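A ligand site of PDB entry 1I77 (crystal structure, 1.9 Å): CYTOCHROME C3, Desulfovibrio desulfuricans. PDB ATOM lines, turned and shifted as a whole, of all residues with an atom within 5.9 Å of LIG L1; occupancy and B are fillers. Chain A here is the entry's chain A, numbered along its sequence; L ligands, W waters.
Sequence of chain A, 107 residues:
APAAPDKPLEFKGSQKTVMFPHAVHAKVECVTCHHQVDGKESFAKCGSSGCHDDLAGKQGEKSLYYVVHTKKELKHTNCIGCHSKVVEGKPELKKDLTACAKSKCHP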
ATOM      1  N   ALA A   1       1.561  -5.529 -11.986  1.00  0.00           N
ATOM      2  CA  ALA A   1       0.116  -5.164 -12.093  1.00  0.00           C
ATOM      3  C   ALA A   1      -0.250  -4.202 -10.978  1.00  0.00           C
ATOM      4  O   ALA A   1       0.466  -4.104  -9.977  1.00  0.00           O
ATOM      5  CB  ALA A   1      -0.738  -6.423 -11.991  1.00  0.00           C
ATOM      6  N   PRO A   2      -1.362  -3.464 -11.138  1.00  0.00           N
ATOM      7  CA  PRO A   2      -1.754  -2.519 -10.086  1.00  0.00           C
ATOM      8  C   PRO A   2      -2.074  -3.264  -8.802  1.00  0.00           C
ATOM      9  O   PRO A   2      -2.140  -4.502  -8.777  1.00  0.00           O
ATOM     10  CB  PRO A   2      -2.989  -1.841 -10.685  1.00  0.00           C
ATOM     11  CG  PRO A   2      -3.596  -2.941 -11.509  1.00  0.00           C
ATOM     12  CD  PRO A   2      -2.378  -3.515 -12.197  1.00  0.00           C
ATOM     13  N   ALA A   3      -2.263  -2.525  -7.714  1.00  0.00           N
ATOM     14  CA  ALA A   3      -2.582  -3.134  -6.430  1.00  0.00           C
ATOM     15  C   ALA A   3      -4.086  -3.423  -6.369  1.00  0.00           C
ATOM     16  O   ALA A   3      -4.884  -2.716  -6.972  1.00  0.00           O
ATOM     17  CB  ALA A   3      -2.177  -2.196  -5.296  1.00  0.00           C
ATOM     18  N   ALA A   4      -4.460  -4.477  -5.648  1.00  0.00           N
ATOM     19  CA  ALA A   4      -5.879  -4.791  -5.522  1.00  0.00           C
ATOM     20  C   ALA A   4      -6.516  -3.805  -4.548  1.00  0.00           C
ATOM     21  O   ALA A   4      -5.988  -3.579  -3.460  1.00  0.00           O
ATOM     22  CB  ALA A   4      -6.049  -6.215  -4.991  1.00  0.00           C
ATOM     23  N   PRO A   5      -7.650  -3.189  -4.929  1.00  0.00           N
ATOM     24  CA  PRO A   5      -8.343  -2.219  -4.066  1.00  0.00           C
ATOM     25  C   PRO A   5      -8.566  -2.763  -2.657  1.00  0.00           C
ATOM     26  O   PRO A   5      -8.908  -3.936  -2.489  1.00  0.00           O
ATOM     27  CB  PRO A   5      -9.657  -1.982  -4.800  1.00  0.00           C
ATOM     28  CG  PRO A   5      -9.252  -2.100  -6.229  1.00  0.00           C
ATOM     29  CD  PRO A   5      -8.320  -3.299  -6.236  1.00  0.00           C
ATOM     30  N   LEU A   9     -15.833  -2.023  -3.577  1.00  0.00           N
ATOM     31  CA  LEU A   9     -16.099  -1.012  -4.581  1.00  0.00           C
ATOM     32  C   LEU A   9     -17.457  -1.231  -5.236  1.00  0.00           C
ATOM     33  O   LEU A   9     -18.051  -2.322  -5.159  1.00  0.00           O
ATOM     34  CB  LEU A   9     -14.982  -0.998  -5.625  1.00  0.00           C
ATOM     35  CG  LEU A   9     -14.520  -2.318  -6.232  1.00  0.00           C
ATOM     36  CD1 LEU A   9     -15.560  -2.803  -7.226  1.00  0.00           C
ATOM     37  CD2 LEU A   9     -13.177  -2.120  -6.920  1.00  0.00           C
ATOM     38  N   GLU A  10     -17.973  -0.182  -5.850  1.00  0.00           N
ATOM     39  CA  GLU A  10     -19.264  -0.262  -6.504  1.00  0.00           C
ATOM     40  C   GLU A  10     -19.116  -0.919  -7.869  1.00  0.00           C
ATOM     41  O   GLU A  10     -18.401  -0.403  -8.735  1.00  0.00           O
ATOM     42  CB  GLU A  10     -19.868   1.134  -6.646  1.00  0.00           C
ATOM     43  CG  GLU A  10     -20.039   1.889  -5.316  1.00  0.00           C
ATOM     44  CD  GLU A  10     -20.849   3.186  -5.454  1.00  0.00           C
ATOM     45  OE1 GLU A  10     -20.644   3.930  -6.439  1.00  0.00           O
ATOM     46  OE2 GLU A  10     -21.686   3.475  -4.579  1.00  0.00           O
ATOM     47  N   PHE A  11     -19.754  -2.071  -8.046  1.00  0.00           N
ATOM     48  CA  PHE A  11     -19.727  -2.798  -9.315  1.00  0.00           C
ATOM     49  C   PHE A  11     -21.164  -2.588  -9.777  1.00  0.00           C
ATOM     50  O   PHE A  11     -22.100  -3.202  -9.260  1.00  0.00           O
ATOM     51  CB  PHE A  11     -19.397  -4.274  -9.061  1.00  0.00           C
ATOM     52  CG  PHE A  11     -19.179  -5.100 -10.308  1.00  0.00           C
ATOM     53  CD1 PHE A  11     -18.866  -4.501 -11.527  1.00  0.00           C
ATOM     54  CD2 PHE A  11     -19.309  -6.500 -10.265  1.00  0.00           C
ATOM     55  CE1 PHE A  11     -18.674  -5.282 -12.697  1.00  0.00           C
ATOM     56  CE2 PHE A  11     -19.112  -7.281 -11.413  1.00  0.00           C
ATOM     57  CZ  PHE A  11     -18.800  -6.681 -12.633  1.00  0.00           C
ATOM     58  N   LYS A  12     -21.321  -1.702 -10.754  1.00  0.00           N
ATOM     59  CA  LYS A  12     -22.636  -1.283 -11.235  1.00  0.00           C
ATOM     60  C   LYS A  12     -23.209  -1.778 -12.545  1.00  0.00           C
ATOM     61  O   LYS A  12     -22.492  -2.032 -13.506  1.00  0.00           O
ATOM     62  CB  LYS A  12     -22.680   0.249 -11.318  1.00  0.00           C
ATOM     63  CG  LYS A  12     -22.230   1.000 -10.065  1.00  0.00           C
ATOM     64  CD  LYS A  12     -22.271   2.496 -10.348  1.00  0.00           C
ATOM     65  CE  LYS A  12     -21.980   3.332  -9.129  1.00  0.00           C
ATOM     66  NZ  LYS A  12     -22.120   4.795  -9.441  1.00  0.00           N
ATOM     67  N   PHE A  20     -18.526  -4.961  -4.334  1.00  0.00           N
ATOM     68  CA  PHE A  20     -17.575  -6.039  -4.577  1.00  0.00           C
ATOM     69  C   PHE A  20     -16.319  -5.947  -3.710  1.00  0.00           C
ATOM     70  O   PHE A  20     -15.548  -4.993  -3.830  1.00  0.00           O
ATOM     71  CB  PHE A  20     -17.154  -6.062  -6.043  1.00  0.00           C
ATOM     72  CG  PHE A  20     -16.124  -7.117  -6.320  1.00  0.00           C
ATOM     73  CD1 PHE A  20     -16.503  -8.448  -6.429  1.00  0.00           C
ATOM     74  CD2 PHE A  20     -14.780  -6.789  -6.327  1.00  0.00           C
ATOM     75  CE1 PHE A  20     -15.548  -9.453  -6.523  1.00  0.00           C
ATOM     76  CE2 PHE A  20     -13.802  -7.797  -6.416  1.00  0.00           C
ATOM     77  CZ  PHE A  20     -14.199  -9.125  -6.507  1.00  0.00           C
ATOM     78  N   HIS A  22     -12.576  -7.232  -2.644  1.00  0.00           N
ATOM     79  CA  HIS A  22     -11.420  -8.007  -3.090  1.00  0.00           C
ATOM     80  C   HIS A  22     -10.841  -8.850  -1.954  1.00  0.00           C
ATOM     81  O   HIS A  22     -10.403  -9.986  -2.176  1.00  0.00           O
ATOM     82  CB  HIS A  22     -10.309  -7.097  -3.613  1.00  0.00           C
ATOM     83  CG  HIS A  22     -10.475  -6.669  -5.035  1.00  0.00           C
ATOM     84  ND1 HIS A  22     -11.308  -5.651  -5.433  1.00  0.00           N
ATOM     85  CD2 HIS A  22      -9.898  -7.138  -6.168  1.00  0.00           C
ATOM     86  CE1 HIS A  22     -11.192  -5.529  -6.775  1.00  0.00           C
ATOM     87  NE2 HIS A  22     -10.343  -6.422  -7.251  1.00  0.00           N
ATOM     88  N   HIS A  25     -11.721 -12.388  -1.671  1.00  0.00           N
ATOM     89  CA  HIS A  25     -11.294 -13.198  -2.811  1.00  0.00           C
ATOM     90  C   HIS A  25      -9.773 -13.210  -2.947  1.00  0.00           C
ATOM     91  O   HIS A  25      -9.268 -13.455  -4.033  1.00  0.00           O
ATOM     92  CB  HIS A  25     -11.875 -12.648  -4.123  1.00  0.00           C
ATOM     93  CG  HIS A  25     -13.367 -12.664  -4.175  1.00  0.00           C
ATOM     94  ND1 HIS A  25     -14.171 -11.628  -3.766  1.00  0.00           N
ATOM     95  CD2 HIS A  25     -14.207 -13.655  -4.566  1.00  0.00           C
ATOM     96  CE1 HIS A  25     -15.447 -12.010  -3.933  1.00  0.00           C
ATOM     97  NE2 HIS A  25     -15.521 -13.228  -4.413  1.00  0.00           N
ATOM     98  N   VAL A  28      -7.980 -16.096  -4.715  1.00  0.00           N
ATOM     99  CA  VAL A  28      -8.301 -16.254  -6.125  1.00  0.00           C
ATOM    100  C   VAL A  28      -7.312 -15.419  -6.954  1.00  0.00           C
ATOM    101  O   VAL A  28      -7.178 -14.211  -6.715  1.00  0.00           O
ATOM    102  CB  VAL A  28      -9.752 -15.750  -6.402  1.00  0.00           C
ATOM    103  CG1 VAL A  28     -10.140 -15.907  -7.867  1.00  0.00           C
ATOM    104  CG2 VAL A  28     -10.737 -16.527  -5.515  1.00  0.00           C
ATOM    105  N   GLU A  29      -6.631 -16.047  -7.913  1.00  0.00           N
ATOM    106  CA  GLU A  29      -5.674 -15.303  -8.752  1.00  0.00           C
ATOM    107  C   GLU A  29      -6.405 -14.182  -9.501  1.00  0.00           C
ATOM    108  O   GLU A  29      -7.519 -14.387  -9.979  1.00  0.00           O
ATOM    109  CB  GLU A  29      -5.021 -16.234  -9.772  1.00  0.00           C
ATOM    110  CG  GLU A  29      -4.111 -17.286  -9.171  1.00  0.00           C
ATOM    111  CD  GLU A  29      -3.579 -18.237 -10.238  1.00  0.00           C
ATOM    112  OE1 GLU A  29      -3.084 -17.751 -11.273  1.00  0.00           O
ATOM    113  OE2 GLU A  29      -3.645 -19.467 -10.034  1.00  0.00           O
ATOM    114  N   CYS A  30      -5.760 -13.036  -9.618  1.00  0.00           N
ATOM    115  CA  CYS A  30      -6.350 -11.895 -10.305  1.00  0.00           C
ATOM    116  C   CYS A  30      -6.960 -12.244 -11.656  1.00  0.00           C
ATOM    117  O   CYS A  30      -8.094 -11.864 -11.955  1.00  0.00           O
ATOM    118  CB  CYS A  30      -5.305 -10.813 -10.553  1.00  0.00           C
ATOM    119  SG  CYS A  30      -4.322 -10.348  -9.117  1.00  0.00           S
ATOM    120  N   VAL A  31      -6.173 -12.949 -12.467  1.00  0.00           N
ATOM    121  CA  VAL A  31      -6.591 -13.314 -13.820  1.00  0.00           C
ATOM    122  C   VAL A  31      -7.870 -14.133 -13.918  1.00  0.00           C
ATOM    123  O   VAL A  31      -8.523 -14.159 -14.961  1.00  0.00           O
ATOM    124  CB  VAL A  31      -5.431 -14.051 -14.543  1.00  0.00           C
ATOM    125  CG1 VAL A  31      -5.126 -15.371 -13.852  1.00  0.00           C
ATOM    126  CG2 VAL A  31      -5.766 -14.248 -16.018  1.00  0.00           C
ATOM    127  N   THR A  32      -8.252 -14.780 -12.834  1.00  0.00           N
ATOM    128  CA  THR A  32      -9.490 -15.573 -12.827  1.00  0.00           C
ATOM    129  C   THR A  32     -10.672 -14.680 -13.259  1.00  0.00           C
ATOM    130  O   THR A  32     -11.542 -15.092 -14.043  1.00  0.00           O
ATOM    131  CB  THR A  32      -9.776 -16.107 -11.400  1.00  0.00           C
ATOM    132  OG1 THR A  32      -8.692 -16.941 -10.972  1.00  0.00           O
ATOM    133  CG2 THR A  32     -11.058 -16.905 -11.388  1.00  0.00           C
ATOM    134  N   CYS A  33     -10.691 -13.461 -12.732  1.00  0.00           N
ATOM    135  CA  CYS A  33     -11.752 -12.496 -13.027  1.00  0.00           C
ATOM    136  C   CYS A  33     -11.296 -11.481 -14.060  1.00  0.00           C
ATOM    137  O   CYS A  33     -12.009 -11.212 -15.024  1.00  0.00           O
ATOM    138  CB  CYS A  33     -12.139 -11.752 -11.743  1.00  0.00           C
ATOM    139  SG  CYS A  33     -12.644 -12.854 -10.405  1.00  0.00           S
ATOM    140  N   HIS A  34     -10.111 -10.914 -13.860  1.00  0.00           N
ATOM    141  CA  HIS A  34      -9.564  -9.937 -14.802  1.00  0.00           C
ATOM    142  C   HIS A  34      -8.882 -10.741 -15.908  1.00  0.00           C
ATOM    143  O   HIS A  34      -7.660 -10.814 -15.995  1.00  0.00           O
ATOM    144  CB  HIS A  34      -8.565  -9.033 -14.091  1.00  0.00           C
ATOM    145  CG  HIS A  34      -9.174  -8.175 -13.020  1.00  0.00           C
ATOM    146  ND1 HIS A  34      -9.956  -7.068 -13.265  1.00  0.00           N
ATOM    147  CD2 HIS A  34      -9.095  -8.262 -11.664  1.00  0.00           C
ATOM    148  CE1 HIS A  34     -10.319  -6.524 -12.096  1.00  0.00           C
ATOM    149  NE2 HIS A  34      -9.829  -7.209 -11.077  1.00  0.00           N
ATOM    150  N   PHE A  43      -6.885  -4.821 -16.504  1.00  0.00           N
ATOM    151  CA  PHE A  43      -7.598  -4.525 -15.281  1.00  0.00           C
ATOM    152  C   PHE A  43      -8.629  -3.430 -15.492  1.00  0.00           C
ATOM    153  O   PHE A  43      -9.063  -2.797 -14.543  1.00  0.00           O
ATOM    154  CB  PHE A  43      -6.629  -4.117 -14.169  1.00  0.00           C
ATOM    155  CG  PHE A  43      -5.717  -5.226 -13.741  1.00  0.00           C
ATOM    156  CD1 PHE A  43      -4.500  -5.425 -14.363  1.00  0.00           C
ATOM    157  CD2 PHE A  43      -6.114  -6.114 -12.736  1.00  0.00           C
ATOM    158  CE1 PHE A  43      -3.687  -6.498 -14.006  1.00  0.00           C
ATOM    159  CE2 PHE A  43      -5.313  -7.176 -12.363  1.00  0.00           C
ATOM    160  CZ  PHE A  43      -4.087  -7.372 -13.005  1.00  0.00           C
ATOM    161  N   ALA A  44      -9.029  -3.212 -16.734  1.00  0.00           N
ATOM    162  CA  ALA A  44     -10.040  -2.196 -17.035  1.00  0.00           C
ATOM    163  C   ALA A  44     -11.394  -2.662 -16.490  1.00  0.00           C
ATOM    164  O   ALA A  44     -11.613  -3.866 -16.269  1.00  0.00           O
ATOM    165  CB  ALA A  44     -10.138  -1.958 -18.536  1.00  0.00           C
ATOM    166  N   LYS A  45     -12.301  -1.721 -16.272  1.00  0.00           N
ATOM    167  CA  LYS A  45     -13.627  -2.049 -15.753  1.00  0.00           C
ATOM    168  C   LYS A  45     -14.352  -2.954 -16.754  1.00  0.00           C
ATOM    169  O   LYS A  45     -14.250  -2.763 -17.971  1.00  0.00           O
ATOM    170  CB  LYS A  45     -14.432  -0.773 -15.481  1.00  0.00           C
ATOM    171  CG  LYS A  45     -13.896   0.037 -14.316  1.00  0.00           C
ATOM    172  CD  LYS A  45     -14.923   1.079 -13.875  1.00  0.00           C
ATOM    173  CE  LYS A  45     -14.600   1.656 -12.496  1.00  0.00           C
ATOM    174  NZ  LYS A  45     -13.356   2.487 -12.483  1.00  0.00           N
ATOM    175  N   CYS A  46     -15.096  -3.931 -16.219  1.00  0.00           N
ATOM    176  CA  CYS A  46     -15.799  -4.911 -17.044  1.00  0.00           C
ATOM    177  C   CYS A  46     -16.711  -4.272 -18.093  1.00  0.00           C
ATOM    178  O   CYS A  46     -16.736  -4.702 -19.239  1.00  0.00           O
ATOM    179  CB  CYS A  46     -16.597  -5.872 -16.142  1.00  0.00           C
ATOM    180  SG  CYS A  46     -15.660  -6.484 -14.683  1.00  0.00           S
ATOM    181  N   GLY A  47     -17.446  -3.249 -17.689  1.00  0.00           N
ATOM    182  CA  GLY A  47     -18.377  -2.600 -18.606  1.00  0.00           C
ATOM    183  C   GLY A  47     -17.907  -1.357 -19.346  1.00  0.00           C
ATOM    184  O   GLY A  47     -18.750  -0.599 -19.845  1.00  0.00           O
HETATM  185  C1  LIG L   1     -11.776  -3.999  -9.892  1.00  0.00           C
HETATM  186  C2  LIG L   1      -7.197  -5.234  -9.338  1.00  0.00           C
HETATM  187  C3  LIG L   1      -8.489  -9.740  -8.218  1.00  0.00           C
HETATM  188  C4  LIG L   1     -12.910  -8.639  -9.680  1.00  0.00           C
HETATM  189  C5  LIG L   1     -10.393  -3.914  -9.764  1.00  0.00           C
HETATM  190  C6  LIG L   1      -9.606  -2.745  -9.947  1.00  0.00           C
HETATM  191  C7  LIG L   1      -8.313  -3.092  -9.873  1.00  0.00           C
HETATM  192  C8  LIG L   1      -8.310  -4.490  -9.616  1.00  0.00           C
HETATM  193  C9  LIG L   1      -7.111  -2.147  -9.881  1.00  0.00           C
HETATM  194  C10 LIG L   1     -10.161  -1.327 -10.044  1.00  0.00           C
HETATM  195  C11 LIG L   1     -10.549  -1.026 -11.469  1.00  0.00           C
HETATM  196  C12 LIG L   1     -10.927   0.423 -11.649  1.00  0.00           C
HETATM  197  O1  LIG L   1     -10.676   0.963 -12.745  1.00  0.00           O
HETATM  198  O2  LIG L   1     -11.481   1.031 -10.693  1.00  0.00           O
HETATM  199  C13 LIG L   1      -7.149  -6.568  -8.954  1.00  0.00           C
HETATM  200  C14 LIG L   1      -5.923  -7.275  -8.709  1.00  0.00           C
HETATM  201  C15 LIG L   1      -6.250  -8.547  -8.327  1.00  0.00           C
HETATM  202  C16 LIG L   1      -7.712  -8.607  -8.434  1.00  0.00           C
HETATM  203  C17 LIG L   1      -4.521  -6.745  -9.042  1.00  0.00           C
HETATM  204  C18 LIG L   1      -5.399  -9.570  -7.883  1.00  0.00           C
HETATM  205  C19 LIG L   1      -4.603  -9.446  -6.684  1.00  0.00           C
HETATM  206  C20 LIG L   1      -9.839  -9.816  -8.449  1.00  0.00           C
HETATM  207  C21 LIG L   1     -10.587 -11.063  -8.405  1.00  0.00           C
HETATM  208  C22 LIG L   1     -11.847 -10.783  -8.877  1.00  0.00           C
HETATM  209  C23 LIG L   1     -11.826  -9.344  -9.227  1.00  0.00           C
HETATM  210  C24 LIG L   1      -9.971 -12.403  -8.034  1.00  0.00           C
HETATM  211  C25 LIG L   1     -12.931 -11.651  -9.009  1.00  0.00           C
HETATM  212  C26 LIG L   1     -13.259 -12.592  -8.018  1.00  0.00           C
HETATM  213  C27 LIG L   1     -13.017  -7.278  -9.796  1.00  0.00           C
HETATM  214  C28 LIG L   1     -14.261  -6.546 -10.116  1.00  0.00           C
HETATM  215  C29 LIG L   1     -13.949  -5.256 -10.166  1.00  0.00           C
HETATM  216  C30 LIG L   1     -12.534  -5.169  -9.885  1.00  0.00           C
HETATM  217  C31 LIG L   1     -15.629  -7.152 -10.368  1.00  0.00           C
HETATM  218  C32 LIG L   1     -14.884  -4.125 -10.563  1.00  0.00           C
HETATM  219  C33 LIG L   1     -14.742  -3.758 -12.039  1.00  0.00           C
HETATM  220  C34 LIG L   1     -15.860  -2.832 -12.512  1.00  0.00           C
HETATM  221  O3  LIG L   1     -16.415  -2.105 -11.677  1.00  0.00           O
HETATM  222  O4  LIG L   1     -16.179  -2.830 -13.716  1.00  0.00           O
HETATM  223  N1  LIG L   1      -9.592  -4.990  -9.547  1.00  0.00           N
HETATM  224  N2  LIG L   1      -8.247  -7.406  -8.833  1.00  0.00           N
HETATM  225  N3  LIG L   1     -10.608  -8.773  -8.938  1.00  0.00           N
HETATM  226  N4  LIG L   1     -11.982  -6.423  -9.657  1.00  0.00           N
HETATM  227 FE1  LIG L   1     -10.116  -6.881  -9.234  1.00  0.00          FE
HETATM  228  C1  LG2 L   2     -17.613 -14.327  -1.463  1.00  0.00           C
HETATM  229  C2  LG2 L   2     -19.127 -11.450  -5.011  1.00  0.00           C
HETATM  230  C3  LG2 L   2     -16.520 -14.025  -8.127  1.00  0.00           C
HETATM  231  C4  LG2 L   2     -15.369 -17.132  -4.691  1.00  0.00           C
HETATM  232  C5  LG2 L   2     -18.241 -13.323  -2.158  1.00  0.00           C
HETATM  233  C6  LG2 L   2     -19.104 -12.286  -1.559  1.00  0.00           C
HETATM  234  C7  LG2 L   2     -19.523 -11.499  -2.553  1.00  0.00           C
HETATM  235  C8  LG2 L   2     -18.968 -12.028  -3.766  1.00  0.00           C
HETATM  236  C9  LG2 L   2     -20.421 -10.273  -2.388  1.00  0.00           C
HETATM  237  C10 LG2 L   2     -19.555 -12.207  -0.115  1.00  0.00           C
HETATM  238  C11 LG2 L   2     -18.617 -11.351   0.705  1.00  0.00           C
HETATM  239  C12 LG2 L   2     -18.980 -11.341   2.196  1.00  0.00           C
HETATM  240  O1  LG2 L   2     -18.838 -12.396   2.851  1.00  0.00           O
HETATM  241  O2  LG2 L   2     -19.414 -10.284   2.698  1.00  0.00           O
HETATM  242  C13 LG2 L   2     -18.542 -11.932  -6.190  1.00  0.00           C
HETATM  243  C14 LG2 L   2     -18.690 -11.269  -7.480  1.00  0.00           C
HETATM  244  C15 LG2 L   2     -17.961 -11.997  -8.378  1.00  0.00           C
HETATM  245  C16 LG2 L   2     -17.346 -13.101  -7.592  1.00  0.00           C
HETATM  246  C17 LG2 L   2     -19.645 -10.087  -7.737  1.00  0.00           C
HETATM  247  C18 LG2 L   2     -17.751 -11.775  -9.756  1.00  0.00           C
HETATM  248  C19 LG2 L   2     -17.107 -10.588 -10.224  1.00  0.00           C
HETATM  249  C20 LG2 L   2     -15.962 -15.070  -7.453  1.00  0.00           C
HETATM  250  C21 LG2 L   2     -15.185 -16.106  -8.122  1.00  0.00           C
HETATM  251  C22 LG2 L   2     -14.933 -17.054  -7.172  1.00  0.00           C
HETATM  252  C23 LG2 L   2     -15.502 -16.535  -5.937  1.00  0.00           C
HETATM  253  C24 LG2 L   2     -14.798 -16.132  -9.603  1.00  0.00           C
HETATM  254  C25 LG2 L   2     -14.297 -18.322  -7.318  1.00  0.00           C
HETATM  255  C26 LG2 L   2     -13.195 -18.517  -8.195  1.00  0.00           C
HETATM  256  C27 LG2 L   2     -15.895 -16.644  -3.524  1.00  0.00           C
HETATM  257  C28 LG2 L   2     -15.663 -17.247  -2.184  1.00  0.00           C
HETATM  258  C29 LG2 L   2     -16.260 -16.397  -1.320  1.00  0.00           C
HETATM  259  C30 LG2 L   2     -16.866 -15.340  -2.049  1.00  0.00           C
HETATM  260  C31 LG2 L   2     -14.803 -18.473  -1.857  1.00  0.00           C
HETATM  261  C32 LG2 L   2     -16.205 -16.427   0.194  1.00  0.00           C
HETATM  262  C33 LG2 L   2     -17.122 -17.489   0.735  1.00  0.00           C
HETATM  263  C34 LG2 L   2     -17.090 -17.551   2.255  1.00  0.00           C
HETATM  264  O3  LG2 L   2     -17.650 -16.641   2.895  1.00  0.00           O
HETATM  265  O4  LG2 L   2     -16.510 -18.510   2.790  1.00  0.00           O
HETATM  266  N1  LG2 L   2     -18.188 -13.159  -3.525  1.00  0.00           N
HETATM  267  N2  LG2 L   2     -17.688 -13.033  -6.253  1.00  0.00           N
HETATM  268  N3  LG2 L   2     -16.171 -15.338  -6.125  1.00  0.00           N
HETATM  269  N4  LG2 L   2     -16.617 -15.471  -3.418  1.00  0.00           N
HETATM  270 FE1  LG2 L   2     -17.175 -14.259  -4.789  1.00  0.00          FE
HETATM  271  C1  LG3 L   3     -15.319 -12.712 -22.261  1.00  0.00           C
HETATM  272  C2  LG3 L   3     -16.147 -11.462 -17.667  1.00  0.00           C
HETATM  273  C3  LG3 L   3     -13.471  -7.526 -18.384  1.00  0.00           C
HETATM  274  C4  LG3 L   3     -13.673  -8.246 -23.124  1.00  0.00           C
HETATM  275  C5  LG3 L   3     -15.672 -12.782 -20.903  1.00  0.00           C
HETATM  276  C6  LG3 L   3     -16.263 -13.968 -20.276  1.00  0.00           C
HETATM  277  C7  LG3 L   3     -16.516 -13.612 -18.998  1.00  0.00           C
HETATM  278  C8  LG3 L   3     -16.084 -12.201 -18.852  1.00  0.00           C
HETATM  279  C9  LG3 L   3     -16.983 -14.507 -17.823  1.00  0.00           C
HETATM  280  C10 LG3 L   3     -16.527 -15.270 -21.030  1.00  0.00           C
HETATM  281  C11 LG3 L   3     -17.795 -15.059 -21.864  1.00  0.00           C
HETATM  282  C12 LG3 L   3     -18.099 -16.226 -22.805  1.00  0.00           C
HETATM  283  O1  LG3 L   3     -17.380 -17.239 -22.790  1.00  0.00           O
HETATM  284  O2  LG3 L   3     -19.075 -16.115 -23.555  1.00  0.00           O
HETATM  285  C13 LG3 L   3     -15.579 -10.208 -17.491  1.00  0.00           C
HETATM  286  C14 LG3 L   3     -15.515  -9.545 -16.207  1.00  0.00           C
HETATM  287  C15 LG3 L   3     -14.641  -8.482 -16.341  1.00  0.00           C
HETATM  288  C16 LG3 L   3     -14.242  -8.493 -17.762  1.00  0.00           C
HETATM  289  C17 LG3 L   3     -16.396  -9.896 -15.017  1.00  0.00           C
HETATM  290  C18 LG3 L   3     -14.302  -7.520 -15.353  1.00  0.00           C
HETATM  291  C19 LG3 L   3     -13.679  -7.931 -14.140  1.00  0.00           C
HETATM  292  C20 LG3 L   3     -13.298  -7.397 -19.729  1.00  0.00           C
HETATM  293  C21 LG3 L   3     -12.742  -6.220 -20.348  1.00  0.00           C
HETATM  294  C22 LG3 L   3     -12.893  -6.318 -21.703  1.00  0.00           C
HETATM  295  C23 LG3 L   3     -13.526  -7.640 -21.892  1.00  0.00           C
HETATM  296  C24 LG3 L   3     -12.123  -5.087 -19.563  1.00  0.00           C
HETATM  297  C25 LG3 L   3     -12.580  -5.370 -22.711  1.00  0.00           C
HETATM  298  C26 LG3 L   3     -11.243  -4.941 -22.886  1.00  0.00           C
HETATM  299  C27 LG3 L   3     -14.139  -9.538 -23.302  1.00  0.00           C
HETATM  300  C28 LG3 L   3     -14.198 -10.190 -24.578  1.00  0.00           C
HETATM  301  C29 LG3 L   3     -14.586 -11.468 -24.343  1.00  0.00           C
HETATM  302  C30 LG3 L   3     -14.808 -11.585 -22.915  1.00  0.00           C
HETATM  303  C31 LG3 L   3     -13.957  -9.567 -25.965  1.00  0.00           C
HETATM  304  C32 LG3 L   3     -14.723 -12.533 -25.443  1.00  0.00           C
HETATM  305  C33 LG3 L   3     -13.349 -13.144 -25.678  1.00  0.00           C
HETATM  306  C34 LG3 L   3     -12.853 -13.902 -24.477  1.00  0.00           C
HETATM  307  O3  LG3 L   3     -13.551 -14.858 -24.057  1.00  0.00           O
HETATM  308  O4  LG3 L   3     -11.787 -13.563 -23.932  1.00  0.00           O
HETATM  309  N1  LG3 L   3     -15.556 -11.737 -20.012  1.00  0.00           N
HETATM  310  N2  LG3 L   3     -14.831  -9.544 -18.449  1.00  0.00           N
HETATM  311  N3  LG3 L   3     -13.831  -8.234 -20.684  1.00  0.00           N
HETATM  312  N4  LG3 L   3     -14.553 -10.395 -22.266  1.00  0.00           N
HETATM  313 FE1  LG3 L   3     -14.676  -9.985 -20.345  1.00  0.00          FE
HETATM  314  O   HOH W   1     -18.690  -0.682 -12.086  1.00  0.00           O
HETATM  315  O   HOH W   2      -4.841   0.312  -9.415  1.00  0.00           O
HETATM  316  O   HOH W   3     -17.862  -1.772 -15.318  1.00  0.00           O
HETATM  317  O   HOH W   4      -6.909 -11.701  -5.681  1.00  0.00           O
HETATM  318  O   HOH W   5     -15.655   0.254  -9.289  1.00  0.00           O
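NZ of Lys 45 is in salt-bridge range of O2 of LIG L1 (3.0 Å).
NE2 of His 34 is bound to FE1 of LIG L1 (1.9 Å).
The side-chain sulfur of Cys 46 is bonded to a carbon (C18) of LG3 L3 (1.8 Å).
The side-chain sulfur (SG) of Cys 30 is covalently linked to a carbon (C18) of LIG L1 (1.8 Å).
An iron atom (FE1) of LIG L1 is bound by a ring nitrogen (NE2) of His 22, at 2.0 Å.
An iron atom (FE1) of LG2 L2 is bound by a ring nitrogen (NE2) of His 25.
An oxygen (O4) of LIG L1 is in hydrogen-bond range of the backbone NH (N) of Cys 46, at 2.9 Å.
C25 of LIG L1 is bonded to SG of Cys 33, at 1.9 Å.
Water W3 lies within hydrogen-bond range of O4 of LIG L1 (2.6 Å) and N of Gly 47 (2.8 Å).
Water W1 lies within hydrogen-bond range of O3 of LIG L1, N of Lys 12 and O of Glu 10.
Water W5 bridges the backbone carbonyl oxygen of Glu 10 and an oxygen (O3) of LIG L1.
O of Pro 2 touches C17 of LIG L1, at 3.3 Å.
O of Ala 3 touches C9 of LIG L1, 3.7 Å away.
Ala 4 touches LIG L1 (CB to C14, 3.9 Å).
CD of Pro 5 touches C8 of LIG L1, 3.6 Å away.
CD1 of Leu 9 touches C32 of LIG L1, at 3.7 Å.
O of Glu 10 touches O3 of LIG L1, 3.9 Å away.
Phe 11 touches LIG L1 (CD1 to O3, 3.4 Å).
CZ of Phe 20 touches C4 of LIG L1, at 3.5 Å.
CD2 of His 25 touches C26 of LIG L1, 3.7 Å away.
Val 28 touches LIG L1 (CG1 to C24, 3.5 Å).
O of Glu 29 touches C24 of LIG L1, at 3.7 Å.
Phe 43 touches LIG L1.
Hydrophobic or aromatic side chains that line LIG L1: Pro 2, Ala 4, Pro 5, Leu 9, Phe 11, Phe 20, His 22, His 25, Val 28, His 34 and Phe 43.
Within 4 Å of LIG L1: Pro 2, Ala 3, Ala 4, Pro 5, Leu 9, Glu 10, Phe 11, Phe 20, His 22, His 25, Val 28, Glu 29, Cys 30, Cys 33, His 34, Phe 43, Lys 45 and Cys 46.
Along chain A the residues within 4 Å of LIG L1 span positions 2 to 46.
The backbone NH (N) of Phe 20 sits at hydrogen-bond distance from the backbone carbonyl oxygen (O) of Leu 9.
OE1 of Glu 10 lies within salt-bridge range of NZ of Lys 12, at 3.5 Å.
O of Glu 29 lies within hydrogen-bond range of OG1 of Thr 32.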
